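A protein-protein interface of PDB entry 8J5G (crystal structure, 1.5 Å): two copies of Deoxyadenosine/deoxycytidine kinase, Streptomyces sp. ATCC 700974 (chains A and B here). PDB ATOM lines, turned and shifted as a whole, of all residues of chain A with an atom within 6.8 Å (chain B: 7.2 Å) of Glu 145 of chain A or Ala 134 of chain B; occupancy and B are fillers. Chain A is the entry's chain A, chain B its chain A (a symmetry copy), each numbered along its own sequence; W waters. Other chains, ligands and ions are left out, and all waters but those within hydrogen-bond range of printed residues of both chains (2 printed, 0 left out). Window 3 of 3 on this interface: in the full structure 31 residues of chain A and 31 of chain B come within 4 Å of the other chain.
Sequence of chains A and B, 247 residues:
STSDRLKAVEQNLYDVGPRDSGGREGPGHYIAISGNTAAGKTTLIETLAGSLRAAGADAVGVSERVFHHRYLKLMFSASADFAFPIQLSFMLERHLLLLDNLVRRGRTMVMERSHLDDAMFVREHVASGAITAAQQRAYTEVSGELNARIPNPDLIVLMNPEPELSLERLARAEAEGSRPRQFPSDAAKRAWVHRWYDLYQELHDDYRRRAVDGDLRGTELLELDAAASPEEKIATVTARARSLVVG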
ATOM      1  N   HIS A  95      33.079  -9.041  20.179  1.00  0.00           N
ATOM      2  CA  HIS A  95      31.762  -9.487  19.731  1.00  0.00           C
ATOM      3  C   HIS A  95      31.756  -9.834  18.247  1.00  0.00           C
ATOM      4  O   HIS A  95      31.243 -10.891  17.847  1.00  0.00           O
ATOM      5  CB  HIS A  95      30.717  -8.400  19.994  1.00  0.00           C
ATOM      6  CG  HIS A  95      29.378  -8.742  19.433  1.00  0.00           C
ATOM      7  ND1 HIS A  95      28.487  -9.559  20.098  1.00  0.00           N
ATOM      8  CD2 HIS A  95      28.805  -8.448  18.239  1.00  0.00           C
ATOM      9  CE1 HIS A  95      27.411  -9.727  19.348  1.00  0.00           C
ATOM     10  NE2 HIS A  95      27.579  -9.070  18.214  1.00  0.00           N
ATOM     11  N   THR A 140      26.091  -0.956  29.462  1.00  0.00           N
ATOM     12  CA  THR A 140      25.407  -2.181  29.851  1.00  0.00           C
ATOM     13  C   THR A 140      24.241  -2.480  28.920  1.00  0.00           C
ATOM     14  O   THR A 140      23.972  -3.648  28.612  1.00  0.00           O
ATOM     15  CB  THR A 140      24.949  -2.063  31.303  1.00  0.00           C
ATOM     16  OG1 THR A 140      26.108  -1.907  32.140  1.00  0.00           O
ATOM     17  CG2 THR A 140      24.167  -3.299  31.749  1.00  0.00           C
ATOM     18  N   GLU A 141      23.557  -1.437  28.441  1.00  0.00           N
ATOM     19  CA  GLU A 141      22.437  -1.646  27.527  1.00  0.00           C
ATOM     20  C   GLU A 141      22.928  -2.289  26.235  1.00  0.00           C
ATOM     21  O   GLU A 141      22.347  -3.264  25.746  1.00  0.00           O
ATOM     22  CB  GLU A 141      21.763  -0.307  27.236  1.00  0.00           C
ATOM     23  CG  GLU A 141      20.886   0.208  28.367  1.00  0.00           C
ATOM     24  CD  GLU A 141      19.871  -0.800  28.844  1.00  0.00           C
ATOM     25  OE1 GLU A 141      18.859  -0.999  28.144  1.00  0.00           O
ATOM     26  OE2 GLU A 141      20.090  -1.389  29.930  1.00  0.00           O
ATOM     27  N   VAL A 142      24.012  -1.757  25.667  1.00  0.00           N
ATOM     28  CA  VAL A 142      24.575  -2.343  24.453  1.00  0.00           C
ATOM     29  C   VAL A 142      25.145  -3.728  24.730  1.00  0.00           C
ATOM     30  O   VAL A 142      24.917  -4.668  23.959  1.00  0.00           O
ATOM     31  CB  VAL A 142      25.636  -1.407  23.856  1.00  0.00           C
ATOM     32  CG1 VAL A 142      26.465  -2.145  22.802  1.00  0.00           C
ATOM     33  CG2 VAL A 142      24.955  -0.199  23.241  1.00  0.00           C
ATOM     34  N   SER A 143      25.877  -3.882  25.837  1.00  0.00           N
ATOM     35  CA  SER A 143      26.468  -5.168  26.200  1.00  0.00           C
ATOM     36  C   SER A 143      25.414  -6.264  26.307  1.00  0.00           C
ATOM     37  O   SER A 143      25.635  -7.384  25.839  1.00  0.00           O
ATOM     38  CB  SER A 143      27.239  -5.016  27.522  1.00  0.00           C
ATOM     39  OG  SER A 143      27.843  -6.245  27.913  1.00  0.00           O
ATOM     40  N   GLY A 144      24.258  -5.961  26.905  1.00  0.00           N
ATOM     41  CA  GLY A 144      23.212  -6.966  27.000  1.00  0.00           C
ATOM     42  C   GLY A 144      22.706  -7.411  25.641  1.00  0.00           C
ATOM     43  O   GLY A 144      22.463  -8.604  25.411  1.00  0.00           O
ATOM     44  N   GLU A 145      22.550  -6.464  24.710  1.00  0.00           N
ATOM     45  CA  GLU A 145      22.056  -6.826  23.386  1.00  0.00           C
ATOM     46  C   GLU A 145      23.093  -7.631  22.622  1.00  0.00           C
ATOM     47  O   GLU A 145      22.748  -8.602  21.930  1.00  0.00           O
ATOM     48  CB  GLU A 145      21.664  -5.573  22.600  1.00  0.00           C
ATOM     49  CG  GLU A 145      20.381  -4.898  23.083  1.00  0.00           C
ATOM     50  CD  GLU A 145      19.130  -5.714  22.800  1.00  0.00           C
ATOM     51  OE1 GLU A 145      19.089  -6.404  21.759  1.00  0.00           O
ATOM     52  OE2 GLU A 145      18.184  -5.661  23.619  1.00  0.00           O
ATOM     53  N   LEU A 146      24.367  -7.250  22.737  1.00  0.00           N
ATOM     54  CA  LEU A 146      25.424  -7.967  22.034  1.00  0.00           C
ATOM     55  C   LEU A 146      25.580  -9.375  22.593  1.00  0.00           C
ATOM     56  O   LEU A 146      25.620 -10.359  21.838  1.00  0.00           O
ATOM     57  CB  LEU A 146      26.740  -7.199  22.147  1.00  0.00           C
ATOM     58  CG  LEU A 146      26.823  -5.869  21.401  1.00  0.00           C
ATOM     59  CD1 LEU A 146      28.197  -5.239  21.698  1.00  0.00           C
ATOM     60  CD2 LEU A 146      26.639  -6.049  19.899  1.00  0.00           C
ATOM     61  N   ASN A 147      25.661  -9.487  23.928  1.00  0.00           N
ATOM     62  CA  ASN A 147      25.903 -10.777  24.559  1.00  0.00           C
ATOM     63  C   ASN A 147      24.758 -11.753  24.317  1.00  0.00           C
ATOM     64  O   ASN A 147      24.983 -12.971  24.278  1.00  0.00           O
ATOM     65  CB  ASN A 147      26.141 -10.581  26.054  1.00  0.00           C
ATOM     66  CG  ASN A 147      27.511 -10.013  26.347  1.00  0.00           C
ATOM     67  OD1 ASN A 147      28.300  -9.748  25.441  1.00  0.00           O
ATOM     68  ND2 ASN A 147      27.814  -9.843  27.628  1.00  0.00           N
ATOM     69  N   ALA A 148      23.531 -11.251  24.143  1.00  0.00           N
ATOM     70  CA  ALA A 148      22.405 -12.147  23.875  1.00  0.00           C
ATOM     71  C   ALA A 148      22.552 -12.893  22.550  1.00  0.00           C
ATOM     72  O   ALA A 148      21.871 -13.907  22.348  1.00  0.00           O
ATOM     73  CB  ALA A 148      21.099 -11.351  23.900  1.00  0.00           C
ATOM     74  N   ARG A 149      23.424 -12.440  21.654  1.00  0.00           N
ATOM     75  CA  ARG A 149      23.619 -13.071  20.350  1.00  0.00           C
ATOM     76  C   ARG A 149      24.810 -14.019  20.316  1.00  0.00           C
ATOM     77  O   ARG A 149      25.082 -14.603  19.259  1.00  0.00           O
ATOM     78  CB  ARG A 149      23.804 -12.001  19.258  1.00  0.00           C
ATOM     79  CG  ARG A 149      22.529 -11.568  18.568  1.00  0.00           C
ATOM     80  CD  ARG A 149      21.655 -10.827  19.531  1.00  0.00           C
ATOM     81  NE  ARG A 149      20.465 -10.242  18.923  1.00  0.00           N
ATOM     82  CZ  ARG A 149      19.732  -9.312  19.521  1.00  0.00           C
ATOM     83  NH1 ARG A 149      20.084  -8.803  20.706  1.00  0.00           N
ATOM     84  NH2 ARG A 149      18.619  -8.884  18.929  1.00  0.00           N
ATOM     85  N   ILE A 150      25.509 -14.198  21.432  1.00  0.00           N
ATOM     86  CA  ILE A 150      26.726 -15.000  21.506  1.00  0.00           C
ATOM     87  C   ILE A 150      26.495 -16.125  22.500  1.00  0.00           C
ATOM     88  O   ILE A 150      26.040 -15.863  23.617  1.00  0.00           O
ATOM     89  CB  ILE A 150      27.950 -14.165  21.932  1.00  0.00           C
ATOM     90  CG1 ILE A 150      28.197 -12.976  20.979  1.00  0.00           C
ATOM     91  CG2 ILE A 150      29.191 -15.061  22.074  1.00  0.00           C
ATOM     92  CD1 ILE A 150      28.462 -13.368  19.529  1.00  0.00           C
ATOM     93  N   PHE B  84      23.801  -4.103  13.361  1.00  0.00           N
ATOM     94  CA  PHE B  84      23.925  -3.441  14.663  1.00  0.00           C
ATOM     95  C   PHE B  84      25.383  -3.269  15.065  1.00  0.00           C
ATOM     96  O   PHE B  84      25.812  -2.121  15.284  1.00  0.00           O
ATOM     97  CB  PHE B  84      23.098  -4.202  15.709  1.00  0.00           C
ATOM     98  CG  PHE B  84      23.184  -3.643  17.115  1.00  0.00           C
ATOM     99  CD1 PHE B  84      22.844  -2.318  17.399  1.00  0.00           C
ATOM    100  CD2 PHE B  84      23.564  -4.476  18.169  1.00  0.00           C
ATOM    101  CE1 PHE B  84      22.911  -1.838  18.715  1.00  0.00           C
ATOM    102  CE2 PHE B  84      23.625  -4.011  19.479  1.00  0.00           C
ATOM    103  CZ  PHE B  84      23.298  -2.686  19.752  1.00  0.00           C
ATOM    104  N   ILE B 131      17.803  -4.180  12.264  1.00  0.00           N
ATOM    105  CA  ILE B 131      18.128  -3.796  13.634  1.00  0.00           C
ATOM    106  C   ILE B 131      16.818  -3.683  14.408  1.00  0.00           C
ATOM    107  O   ILE B 131      15.847  -3.100  13.910  1.00  0.00           O
ATOM    108  CB  ILE B 131      18.927  -2.478  13.680  1.00  0.00           C
ATOM    109  CG1 ILE B 131      20.334  -2.696  13.104  1.00  0.00           C
ATOM    110  CG2 ILE B 131      19.031  -1.956  15.113  1.00  0.00           C
ATOM    111  CD1 ILE B 131      21.194  -1.432  13.068  1.00  0.00           C
ATOM    112  N   THR B 132      16.768  -4.291  15.589  1.00  0.00           N
ATOM    113  CA  THR B 132      15.539  -4.267  16.374  1.00  0.00           C
ATOM    114  C   THR B 132      15.384  -2.927  17.087  1.00  0.00           C
ATOM    115  O   THR B 132      16.344  -2.164  17.247  1.00  0.00           O
ATOM    116  CB  THR B 132      15.522  -5.374  17.426  1.00  0.00           C
ATOM    117  OG1 THR B 132      16.483  -5.072  18.450  1.00  0.00           O
ATOM    118  CG2 THR B 132      15.838  -6.740  16.812  1.00  0.00           C
ATOM    119  N   ALA B 133      14.162  -2.659  17.559  1.00  0.00           N
ATOM    120  CA  ALA B 133      13.934  -1.427  18.309  1.00  0.00           C
ATOM    121  C   ALA B 133      14.764  -1.401  19.586  1.00  0.00           C
ATOM    122  O   ALA B 133      15.265  -0.338  19.987  1.00  0.00           O
ATOM    123  CB  ALA B 133      12.450  -1.269  18.634  1.00  0.00           C
ATOM    124  N   ALA B 134      14.914  -2.555  20.248  1.00  0.00           N
ATOM    125  CA  ALA B 134      15.724  -2.616  21.465  1.00  0.00           C
ATOM    126  C   ALA B 134      17.194  -2.331  21.175  1.00  0.00           C
ATOM    127  O   ALA B 134      17.864  -1.633  21.953  1.00  0.00           O
ATOM    128  CB  ALA B 134      15.572  -3.983  22.139  1.00  0.00           C
ATOM    129  N   GLN B 135      17.710  -2.853  20.062  1.00  0.00           N
ATOM    130  CA  GLN B 135      19.072  -2.529  19.654  1.00  0.00           C
ATOM    131  C   GLN B 135      19.210  -1.047  19.350  1.00  0.00           C
ATOM    132  O   GLN B 135      20.195  -0.410  19.756  1.00  0.00           O
ATOM    133  CB  GLN B 135      19.470  -3.362  18.435  1.00  0.00           C
ATOM    134  CG  GLN B 135      19.775  -4.807  18.776  1.00  0.00           C
ATOM    135  CD  GLN B 135      19.948  -5.665  17.543  1.00  0.00           C
ATOM    136  OE1 GLN B 135      19.231  -5.503  16.547  1.00  0.00           O
ATOM    137  NE2 GLN B 135      20.917  -6.574  17.591  1.00  0.00           N
ATOM    138  N   GLN B 136      18.227  -0.465  18.655  1.00  0.00           N
ATOM    139  CA  GLN B 136      18.311   0.965  18.378  1.00  0.00           C
ATOM    140  C   GLN B 136      18.330   1.781  19.665  1.00  0.00           C
ATOM    141  O   GLN B 136      19.086   2.752  19.775  1.00  0.00           O
ATOM    142  CB  GLN B 136      17.155   1.411  17.493  1.00  0.00           C
ATOM    143  CG  GLN B 136      17.242   2.901  17.194  1.00  0.00           C
ATOM    144  CD  GLN B 136      16.134   3.368  16.281  1.00  0.00           C
ATOM    145  OE1 GLN B 136      14.970   3.024  16.478  1.00  0.00           O
ATOM    146  NE2 GLN B 136      16.490   4.180  15.291  1.00  0.00           N
ATOM    147  N   ARG B 137      17.512   1.411  20.657  1.00  0.00           N
ATOM    148  CA  ARG B 137      17.518   2.165  21.910  1.00  0.00           C
ATOM    149  C   ARG B 137      18.876   2.096  22.599  1.00  0.00           C
ATOM    150  O   ARG B 137      19.353   3.108  23.135  1.00  0.00           O
ATOM    151  CB  ARG B 137      16.420   1.666  22.849  1.00  0.00           C
ATOM    152  CG  ARG B 137      15.023   2.072  22.405  1.00  0.00           C
ATOM    153  CD  ARG B 137      13.990   1.799  23.475  1.00  0.00           C
ATOM    154  NE  ARG B 137      13.904   0.386  23.820  1.00  0.00           N
ATOM    155  CZ  ARG B 137      13.156  -0.495  23.169  1.00  0.00           C
ATOM    156  NH1 ARG B 137      12.475  -0.152  22.085  1.00  0.00           N
ATOM    157  NH2 ARG B 137      13.090  -1.748  23.614  1.00  0.00           N
ATOM    158  N   ALA B 138      19.504   0.914  22.612  1.00  0.00           N
ATOM    159  CA  ALA B 138      20.835   0.799  23.207  1.00  0.00           C
ATOM    160  C   ALA B 138      21.842   1.635  22.432  1.00  0.00           C
ATOM    161  O   ALA B 138      22.658   2.356  23.028  1.00  0.00           O
ATOM    162  CB  ALA B 138      21.272  -0.665  23.245  1.00  0.00           C
ATOM    163  N   TYR B 139      21.773   1.583  21.103  1.00  0.00           N
ATOM    164  CA  TYR B 139      22.625   2.426  20.263  1.00  0.00           C
ATOM    165  C   TYR B 139      22.478   3.900  20.624  1.00  0.00           C
ATOM    166  O   TYR B 139      23.470   4.628  20.751  1.00  0.00           O
ATOM    167  CB  TYR B 139      22.267   2.206  18.792  1.00  0.00           C
ATOM    168  CG  TYR B 139      23.003   3.107  17.831  1.00  0.00           C
ATOM    169  CD1 TYR B 139      22.507   4.374  17.509  1.00  0.00           C
ATOM    170  CD2 TYR B 139      24.205   2.710  17.261  1.00  0.00           C
ATOM    171  CE1 TYR B 139      23.187   5.207  16.637  1.00  0.00           C
ATOM    172  CE2 TYR B 139      24.897   3.536  16.386  1.00  0.00           C
ATOM    173  CZ  TYR B 139      24.378   4.784  16.074  1.00  0.00           C
ATOM    174  OH  TYR B 139      25.032   5.609  15.194  1.00  0.00           O
ATOM    175  N   THR B 140      21.231   4.363  20.753  1.00  0.00           N
ATOM    176  CA  THR B 140      20.979   5.776  21.000  1.00  0.00           C
ATOM    177  C   THR B 140      21.516   6.201  22.360  1.00  0.00           C
ATOM    178  O   THR B 140      22.017   7.322  22.510  1.00  0.00           O
ATOM    179  CB  THR B 140      19.481   6.049  20.879  1.00  0.00           C
ATOM    180  OG1 THR B 140      19.066   5.745  19.537  1.00  0.00           O
ATOM    181  CG2 THR B 140      19.148   7.509  21.191  1.00  0.00           C
HETATM  182  O   HOH W   1      23.032  -7.398  19.318  1.00  0.00           O
HETATM  183  O   HOH W   2      17.023  -7.027  20.207  1.00  0.00           O
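Water W2 lies within hydrogen-bond range of OE1 of Glu 145 of chain A (2.7 Å), OG1 of Thr 132 of chain B (2.7 Å) and NH2 of Arg 149 of chain A (2.8 Å).
Water W1 bridges NE2 of Gln 135 of chain B (2.9 Å) and O of Glu 145 of chain A (2.9 Å).
1 position is printed for both chains.
Of the 6 pairs that touch across the chains among the printed residues, none has its exchanged pair printed and touching as well.
Of the 12 printed residues of chain A, 5 touch a printed residue of chain B.
Printed residues of chain A that touch a printed residue of chain B: Glu 141, Val 142, Glu 145, Leu 146 and Arg 149.
Hydrophobic or aromatic side chains of chain A that line the printed part of chain B: Val 142 and Leu 146.
Of the 11 printed residues of chain B, 4 touch a printed residue of chain A.
Of the printed residues of chain B, Glu 145 of chain A touches Ala 134 and Gln 135.
Of chain A, only Glu 145 (3.4 Å) comes within 4 Å of Ala 134 of chain B.
No residue of chain B comes within 4 Å of Gly 144 of chain A.
Of the printed residues of chain B, Arg 149 of chain A touches Gln 135.
Printed residues of chain B within 4 Å of Leu 146 of chain A: Phe 84 (3.7 Å).
Of the printed residues of chain B, Val 142 of chain A touches Ala 138.
Of the printed residues of chain A, Ala 138 of chain B touches Glu 141 (3.8 Å) and Val 142 (3.4 Å).
Of the printed residues of chain A, Phe 84 of chain B touches Leu 146.
Ile 131 of chain B touches none of the printed residues of chain A.
The nearest residue of chain A that does not touch Ala 134 of chain B is Glu 141 of chain A (6.1 Å).
A ring nitrogen (ND1) of His 95 of chain A lies close to the backbone carbonyl oxygen (O) of Leu 146 of chain A, 3.4 Å away.
OE1 of Glu 145 of chain A lies within salt-bridge range of NH1 of Arg 149 of chain A, at 2.8 Å.
The side-chain hydroxyl (OG1) of Thr 132 of chain B sits close to the backbone NH (N) of Ala 134 of chain B, at 3.5 Å.
N of Thr 132 of chain B sits at hydrogen-bond distance from OE1 of Gln 135 of chain B (2.9 Å).
Glu 141 of chain A touches Ala 138 of chain B (O to CB, 3.8 Å).
Ala 138 of chain B touches Val 142 of chain A (O to CG2, 3.4 Å).
Glu 145 of chain A touches Ala 134 of chain B (OE2 to CB, 3.4 Å).
OE1 of Glu 145 of chain A touches CG of Gln 135 of chain B (3.5 Å).
Leu 146 of chain A touches Phe 84 of chain B.
Arg 149 of chain A touches Gln 135 of chain B (NH2 to NE2, 3.5 Å).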
